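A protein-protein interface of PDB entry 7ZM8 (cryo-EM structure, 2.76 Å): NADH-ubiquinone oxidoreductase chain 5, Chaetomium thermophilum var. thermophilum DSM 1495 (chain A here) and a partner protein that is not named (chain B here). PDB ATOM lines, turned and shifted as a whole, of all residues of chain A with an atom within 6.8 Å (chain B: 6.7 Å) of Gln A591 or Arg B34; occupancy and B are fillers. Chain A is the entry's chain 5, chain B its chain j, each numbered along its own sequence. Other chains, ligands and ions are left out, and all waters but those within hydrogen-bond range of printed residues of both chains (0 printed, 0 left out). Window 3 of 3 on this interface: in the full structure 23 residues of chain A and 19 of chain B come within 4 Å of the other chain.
Of chain B, only Arg B34 (3.6 Å), Val B38 (3.7 Å) and Tyr B42 (3.5 Å) come within 4 Å of Gln A591. Of the printed residues of chain B, Ile A592 touches Tyr B42. Thr A593 touches none of the printed residues of chain B. Of the printed residues of chain A, Arg B34 touches Gln A591 (3.6 Å) and Ile A595 (3.4 Å). Of the printed residues of chain A, Ser B39 touches Leu A596. The nearest printed residue of chain B that does not touch Gln A591 is Ser B39 (7.3 Å). The nearest printed residue of chain B that does not touch Leu A596 is Val B38 (4.2 Å).
Tyr B42 touches Leu A588. Gln A591 touches Arg B34 (NE2 to NH2, 3.6 Å). CG1 of Val B38 touches OE1 of Gln A591, 3.7 Å away. Ile A592 touches Tyr B42. CD1 of Ile A595 touches NH2 of Arg B34, at 3.4 Å. Leu A596 touches Ser B39. Leu A596 touches Tyr B42 (CD1 to CG, 3.4 Å).
OE1 of Gln A591 is in hydrogen-bond range of OH of Tyr B42.
The backbone carbonyl oxygen of Ile A592 sits at hydrogen-bond distance from the backbone NH of Asp A597 (2.7 Å). O of Gln A591 sits at hydrogen-bond distance from N of Leu A596 (3.4 Å). The side-chain hydroxyl (OG1) of Thr B32 sits at hydrogen-bond distance from the backbone NH (N) of Arg B34 (3.0 Å).
Along chain A the printed residues that touch a printed residue of chain B span positions 588 to 596. Among the printed residues, no Asp or Glu carboxylate lies within 4 Å of a Lys or Arg side-chain nitrogen of the other chain.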
ATOM      1  N   LEU A 586      -2.897  -7.925 -22.869  1.00  0.00           N
ATOM      2  CA  LEU A 586      -3.270  -9.143 -23.576  1.00  0.00           C
ATOM      3  C   LEU A 586      -2.481 -10.345 -23.077  1.00  0.00           C
ATOM      4  O   LEU A 586      -2.987 -11.470 -23.114  1.00  0.00           O
ATOM      5  CB  LEU A 586      -3.089  -8.968 -25.085  1.00  0.00           C
ATOM      6  CG  LEU A 586      -4.197  -8.286 -25.897  1.00  0.00           C
ATOM      7  CD1 LEU A 586      -5.468  -9.089 -25.812  1.00  0.00           C
ATOM      8  CD2 LEU A 586      -4.467  -6.868 -25.471  1.00  0.00           C
ATOM      9  N   ASN A 587      -1.243 -10.141 -22.624  1.00  0.00           N
ATOM     10  CA  ASN A 587      -0.534 -11.219 -21.944  1.00  0.00           C
ATOM     11  C   ASN A 587      -1.186 -11.557 -20.610  1.00  0.00           C
ATOM     12  O   ASN A 587      -1.304 -12.732 -20.256  1.00  0.00           O
ATOM     13  CB  ASN A 587       0.934 -10.850 -21.725  1.00  0.00           C
ATOM     14  CG  ASN A 587       1.700 -10.692 -23.021  1.00  0.00           C
ATOM     15  OD1 ASN A 587       2.191  -9.612 -23.334  1.00  0.00           O
ATOM     16  ND2 ASN A 587       1.809 -11.775 -23.779  1.00  0.00           N
ATOM     17  N   LEU A 588      -1.602 -10.541 -19.851  1.00  0.00           N
ATOM     18  CA  LEU A 588      -2.224 -10.796 -18.557  1.00  0.00           C
ATOM     19  C   LEU A 588      -3.515 -11.582 -18.714  1.00  0.00           C
ATOM     20  O   LEU A 588      -3.821 -12.456 -17.899  1.00  0.00           O
ATOM     21  CB  LEU A 588      -2.492  -9.485 -17.819  1.00  0.00           C
ATOM     22  CG  LEU A 588      -1.319  -8.685 -17.258  1.00  0.00           C
ATOM     23  CD1 LEU A 588      -1.833  -7.529 -16.434  1.00  0.00           C
ATOM     24  CD2 LEU A 588      -0.397  -9.547 -16.438  1.00  0.00           C
ATOM     25  N   GLY A 589      -4.292 -11.273 -19.746  1.00  0.00           N
ATOM     26  CA  GLY A 589      -5.486 -12.052 -20.011  1.00  0.00           C
ATOM     27  C   GLY A 589      -5.174 -13.495 -20.346  1.00  0.00           C
ATOM     28  O   GLY A 589      -5.875 -14.409 -19.908  1.00  0.00           O
ATOM     29  N   GLY A 590      -4.120 -13.718 -21.131  1.00  0.00           N
ATOM     30  CA  GLY A 590      -3.734 -15.077 -21.468  1.00  0.00           C
ATOM     31  C   GLY A 590      -3.244 -15.871 -20.274  1.00  0.00           C
ATOM     32  O   GLY A 590      -3.572 -17.049 -20.127  1.00  0.00           O
ATOM     33  N   GLN A 591      -2.447 -15.242 -19.409  1.00  0.00           N
ATOM     34  CA  GLN A 591      -1.923 -15.936 -18.235  1.00  0.00           C
ATOM     35  C   GLN A 591      -3.033 -16.325 -17.270  1.00  0.00           C
ATOM     36  O   GLN A 591      -2.988 -17.403 -16.667  1.00  0.00           O
ATOM     37  CB  GLN A 591      -0.889 -15.067 -17.530  1.00  0.00           C
ATOM     38  CG  GLN A 591       0.528 -15.341 -17.959  1.00  0.00           C
ATOM     39  CD  GLN A 591       1.525 -14.961 -16.897  1.00  0.00           C
ATOM     40  OE1 GLN A 591       1.162 -14.401 -15.868  1.00  0.00           O
ATOM     41  NE2 GLN A 591       2.791 -15.269 -17.136  1.00  0.00           N
ATOM     42  N   ILE A 592      -4.024 -15.452 -17.089  1.00  0.00           N
ATOM     43  CA  ILE A 592      -5.167 -15.800 -16.257  1.00  0.00           C
ATOM     44  C   ILE A 592      -5.954 -16.940 -16.887  1.00  0.00           C
ATOM     45  O   ILE A 592      -6.365 -17.883 -16.204  1.00  0.00           O
ATOM     46  CB  ILE A 592      -6.046 -14.560 -16.012  1.00  0.00           C
ATOM     47  CG1 ILE A 592      -5.267 -13.502 -15.232  1.00  0.00           C
ATOM     48  CG2 ILE A 592      -7.311 -14.937 -15.261  1.00  0.00           C
ATOM     49  CD1 ILE A 592      -5.933 -12.161 -15.182  1.00  0.00           C
ATOM     50  N   THR A 593      -6.170 -16.877 -18.200  1.00  0.00           N
ATOM     51  CA  THR A 593      -6.933 -17.919 -18.878  1.00  0.00           C
ATOM     52  C   THR A 593      -6.170 -19.235 -18.910  1.00  0.00           C
ATOM     53  O   THR A 593      -6.730 -20.296 -18.618  1.00  0.00           O
ATOM     54  CB  THR A 593      -7.283 -17.476 -20.297  1.00  0.00           C
ATOM     55  OG1 THR A 593      -7.835 -16.157 -20.270  1.00  0.00           O
ATOM     56  CG2 THR A 593      -8.296 -18.423 -20.911  1.00  0.00           C
ATOM     57  N   LYS A 594      -4.886 -19.189 -19.270  1.00  0.00           N
ATOM     58  CA  LYS A 594      -4.126 -20.419 -19.455  1.00  0.00           C
ATOM     59  C   LYS A 594      -3.684 -21.021 -18.128  1.00  0.00           C
ATOM     60  O   LYS A 594      -3.895 -22.211 -17.883  1.00  0.00           O
ATOM     61  CB  LYS A 594      -2.912 -20.155 -20.339  1.00  0.00           C
ATOM     62  CG  LYS A 594      -3.238 -19.899 -21.787  1.00  0.00           C
ATOM     63  CD  LYS A 594      -1.961 -19.788 -22.594  1.00  0.00           C
ATOM     64  CE  LYS A 594      -1.230 -18.488 -22.307  1.00  0.00           C
ATOM     65  NZ  LYS A 594      -1.808 -17.349 -23.071  1.00  0.00           N
ATOM     66  N   ILE A 595      -3.061 -20.225 -17.266  1.00  0.00           N
ATOM     67  CA  ILE A 595      -2.433 -20.787 -16.078  1.00  0.00           C
ATOM     68  C   ILE A 595      -3.372 -20.816 -14.873  1.00  0.00           C
ATOM     69  O   ILE A 595      -3.196 -21.648 -13.980  1.00  0.00           O
ATOM     70  CB  ILE A 595      -1.137 -20.023 -15.756  1.00  0.00           C
ATOM     71  CG1 ILE A 595      -0.308 -19.829 -17.022  1.00  0.00           C
ATOM     72  CG2 ILE A 595      -0.304 -20.774 -14.738  1.00  0.00           C
ATOM     73  CD1 ILE A 595       0.870 -18.934 -16.837  1.00  0.00           C
ATOM     74  N   LEU A 596      -4.382 -19.959 -14.837  1.00  0.00           N
ATOM     75  CA  LEU A 596      -5.224 -19.961 -13.619  1.00  0.00           C
ATOM     76  C   LEU A 596      -6.562 -20.610 -13.916  1.00  0.00           C
ATOM     77  O   LEU A 596      -6.821 -21.659 -13.333  1.00  0.00           O
ATOM     78  CB  LEU A 596      -5.419 -18.542 -13.084  1.00  0.00           C
ATOM     79  CG  LEU A 596      -4.156 -17.715 -12.882  1.00  0.00           C
ATOM     80  CD1 LEU A 596      -4.521 -16.260 -12.691  1.00  0.00           C
ATOM     81  CD2 LEU A 596      -3.363 -18.225 -11.694  1.00  0.00           C
ATOM     82  N   ASP A 597      -7.367 -20.023 -14.801  1.00  0.00           N
ATOM     83  CA  ASP A 597      -8.748 -20.524 -15.045  1.00  0.00           C
ATOM     84  C   ASP A 597      -8.734 -21.948 -15.573  1.00  0.00           C
ATOM     85  O   ASP A 597      -9.539 -22.756 -15.095  1.00  0.00           O
ATOM     86  CB  ASP A 597      -9.414 -19.752 -16.178  1.00  0.00           C
ATOM     87  CG  ASP A 597      -9.924 -18.381 -15.788  1.00  0.00           C
ATOM     88  OD1 ASP A 597     -10.477 -18.258 -14.683  1.00  0.00           O
ATOM     89  OD2 ASP A 597      -9.775 -17.456 -16.601  1.00  0.00           O
ATOM     90  N   TRP B  31       1.996 -28.917 -11.816  1.00  0.00           N
ATOM     91  CA  TRP B  31       2.509 -27.982 -10.787  1.00  0.00           C
ATOM     92  C   TRP B  31       4.011 -27.885 -10.989  1.00  0.00           C
ATOM     93  O   TRP B  31       4.705 -28.861 -10.677  1.00  0.00           O
ATOM     94  CB  TRP B  31       2.209 -28.459  -9.363  1.00  0.00           C
ATOM     95  CG  TRP B  31       0.821 -28.209  -8.867  1.00  0.00           C
ATOM     96  CD1 TRP B  31      -0.096 -29.145  -8.493  1.00  0.00           C
ATOM     97  CD2 TRP B  31       0.199 -26.931  -8.657  1.00  0.00           C
ATOM     98  NE1 TRP B  31      -1.250 -28.541  -8.080  1.00  0.00           N
ATOM     99  CE2 TRP B  31      -1.101 -27.183  -8.172  1.00  0.00           C
ATOM    100  CE3 TRP B  31       0.606 -25.606  -8.842  1.00  0.00           C
ATOM    101  CZ2 TRP B  31      -1.992 -26.156  -7.868  1.00  0.00           C
ATOM    102  CZ3 TRP B  31      -0.273 -24.592  -8.539  1.00  0.00           C
ATOM    103  CH2 TRP B  31      -1.552 -24.867  -8.056  1.00  0.00           C
ATOM    104  N   THR B  32       4.484 -26.775 -11.528  1.00  0.00           N
ATOM    105  CA  THR B  32       5.891 -26.502 -11.736  1.00  0.00           C
ATOM    106  C   THR B  32       6.313 -25.381 -10.799  1.00  0.00           C
ATOM    107  O   THR B  32       5.511 -24.859 -10.025  1.00  0.00           O
ATOM    108  CB  THR B  32       6.179 -26.135 -13.196  1.00  0.00           C
ATOM    109  OG1 THR B  32       5.704 -24.813 -13.464  1.00  0.00           O
ATOM    110  CG2 THR B  32       5.500 -27.104 -14.136  1.00  0.00           C
ATOM    111  N   LYS B  33       7.595 -25.027 -10.861  1.00  0.00           N
ATOM    112  CA  LYS B  33       8.057 -23.840 -10.158  1.00  0.00           C
ATOM    113  C   LYS B  33       7.475 -22.578 -10.777  1.00  0.00           C
ATOM    114  O   LYS B  33       7.316 -21.564 -10.091  1.00  0.00           O
ATOM    115  CB  LYS B  33       9.584 -23.790 -10.166  1.00  0.00           C
ATOM    116  CG  LYS B  33      10.195 -22.888  -9.108  1.00  0.00           C
ATOM    117  CD  LYS B  33      11.701 -23.078  -9.034  1.00  0.00           C
ATOM    118  CE  LYS B  33      12.312 -22.235  -7.927  1.00  0.00           C
ATOM    119  NZ  LYS B  33      13.787 -22.424  -7.832  1.00  0.00           N
ATOM    120  N   ARG B  34       7.142 -22.626 -12.064  1.00  0.00           N
ATOM    121  CA  ARG B  34       6.618 -21.456 -12.752  1.00  0.00           C
ATOM    122  C   ARG B  34       5.122 -21.295 -12.518  1.00  0.00           C
ATOM    123  O   ARG B  34       4.652 -20.198 -12.205  1.00  0.00           O
ATOM    124  CB  ARG B  34       6.923 -21.557 -14.248  1.00  0.00           C
ATOM    125  CG  ARG B  34       6.738 -20.263 -15.014  1.00  0.00           C
ATOM    126  CD  ARG B  34       6.580 -20.529 -16.499  1.00  0.00           C
ATOM    127  NE  ARG B  34       5.858 -19.460 -17.180  1.00  0.00           N
ATOM    128  CZ  ARG B  34       4.567 -19.512 -17.493  1.00  0.00           C
ATOM    129  NH1 ARG B  34       3.850 -20.584 -17.184  1.00  0.00           N
ATOM    130  NH2 ARG B  34       3.994 -18.490 -18.115  1.00  0.00           N
ATOM    131  N   THR B  35       4.356 -22.377 -12.673  1.00  0.00           N
ATOM    132  CA  THR B  35       2.908 -22.276 -12.539  1.00  0.00           C
ATOM    133  C   THR B  35       2.516 -21.946 -11.107  1.00  0.00           C
ATOM    134  O   THR B  35       1.526 -21.247 -10.872  1.00  0.00           O
ATOM    135  CB  THR B  35       2.239 -23.570 -12.995  1.00  0.00           C
ATOM    136  OG1 THR B  35       2.625 -24.640 -12.130  1.00  0.00           O
ATOM    137  CG2 THR B  35       2.645 -23.906 -14.404  1.00  0.00           C
ATOM    138  N   ALA B  36       3.279 -22.448 -10.138  1.00  0.00           N
ATOM    139  CA  ALA B  36       3.057 -22.074  -8.747  1.00  0.00           C
ATOM    140  C   ALA B  36       3.356 -20.598  -8.514  1.00  0.00           C
ATOM    141  O   ALA B  36       2.635 -19.920  -7.775  1.00  0.00           O
ATOM    142  CB  ALA B  36       3.912 -22.948  -7.834  1.00  0.00           C
ATOM    143  N   LEU B  37       4.424 -20.085  -9.127  1.00  0.00           N
ATOM    144  CA  LEU B  37       4.785 -18.686  -8.935  1.00  0.00           C
ATOM    145  C   LEU B  37       3.716 -17.751  -9.492  1.00  0.00           C
ATOM    146  O   LEU B  37       3.368 -16.749  -8.858  1.00  0.00           O
ATOM    147  CB  LEU B  37       6.136 -18.405  -9.588  1.00  0.00           C
ATOM    148  CG  LEU B  37       6.691 -16.989  -9.422  1.00  0.00           C
ATOM    149  CD1 LEU B  37       6.943 -16.684  -7.954  1.00  0.00           C
ATOM    150  CD2 LEU B  37       7.959 -16.814 -10.235  1.00  0.00           C
ATOM    151  N   VAL B  38       3.192 -18.054 -10.679  1.00  0.00           N
ATOM    152  CA  VAL B  38       2.118 -17.243 -11.241  1.00  0.00           C
ATOM    153  C   VAL B  38       0.836 -17.416 -10.432  1.00  0.00           C
ATOM    154  O   VAL B  38       0.107 -16.450 -10.182  1.00  0.00           O
ATOM    155  CB  VAL B  38       1.914 -17.589 -12.728  1.00  0.00           C
ATOM    156  CG1 VAL B  38       0.634 -16.991 -13.254  1.00  0.00           C
ATOM    157  CG2 VAL B  38       3.082 -17.095 -13.548  1.00  0.00           C
ATOM    158  N   SER B  39       0.543 -18.643 -10.007  1.00  0.00           N
ATOM    159  CA  SER B  39      -0.683 -18.885  -9.257  1.00  0.00           C
ATOM    160  C   SER B  39      -0.648 -18.201  -7.899  1.00  0.00           C
ATOM    161  O   SER B  39      -1.648 -17.618  -7.467  1.00  0.00           O
ATOM    162  CB  SER B  39      -0.906 -20.384  -9.096  1.00  0.00           C
ATOM    163  OG  SER B  39      -0.707 -21.041 -10.331  1.00  0.00           O
ATOM    164  N   TYR B  42      -1.147 -14.241  -8.381  1.00  0.00           N
ATOM    165  CA  TYR B  42      -2.485 -13.803  -8.753  1.00  0.00           C
ATOM    166  C   TYR B  42      -3.503 -14.089  -7.659  1.00  0.00           C
ATOM    167  O   TYR B  42      -4.385 -13.267  -7.394  1.00  0.00           O
ATOM    168  CB  TYR B  42      -2.916 -14.505 -10.033  1.00  0.00           C
ATOM    169  CG  TYR B  42      -2.472 -13.867 -11.321  1.00  0.00           C
ATOM    170  CD1 TYR B  42      -3.053 -12.696 -11.772  1.00  0.00           C
ATOM    171  CD2 TYR B  42      -1.505 -14.465 -12.110  1.00  0.00           C
ATOM    172  CE1 TYR B  42      -2.664 -12.128 -12.958  1.00  0.00           C
ATOM    173  CE2 TYR B  42      -1.109 -13.904 -13.292  1.00  0.00           C
ATOM    174  CZ  TYR B  42      -1.692 -12.737 -13.717  1.00  0.00           C
ATOM    175  OH  TYR B  42      -1.303 -12.169 -14.902  1.00  0.00           O
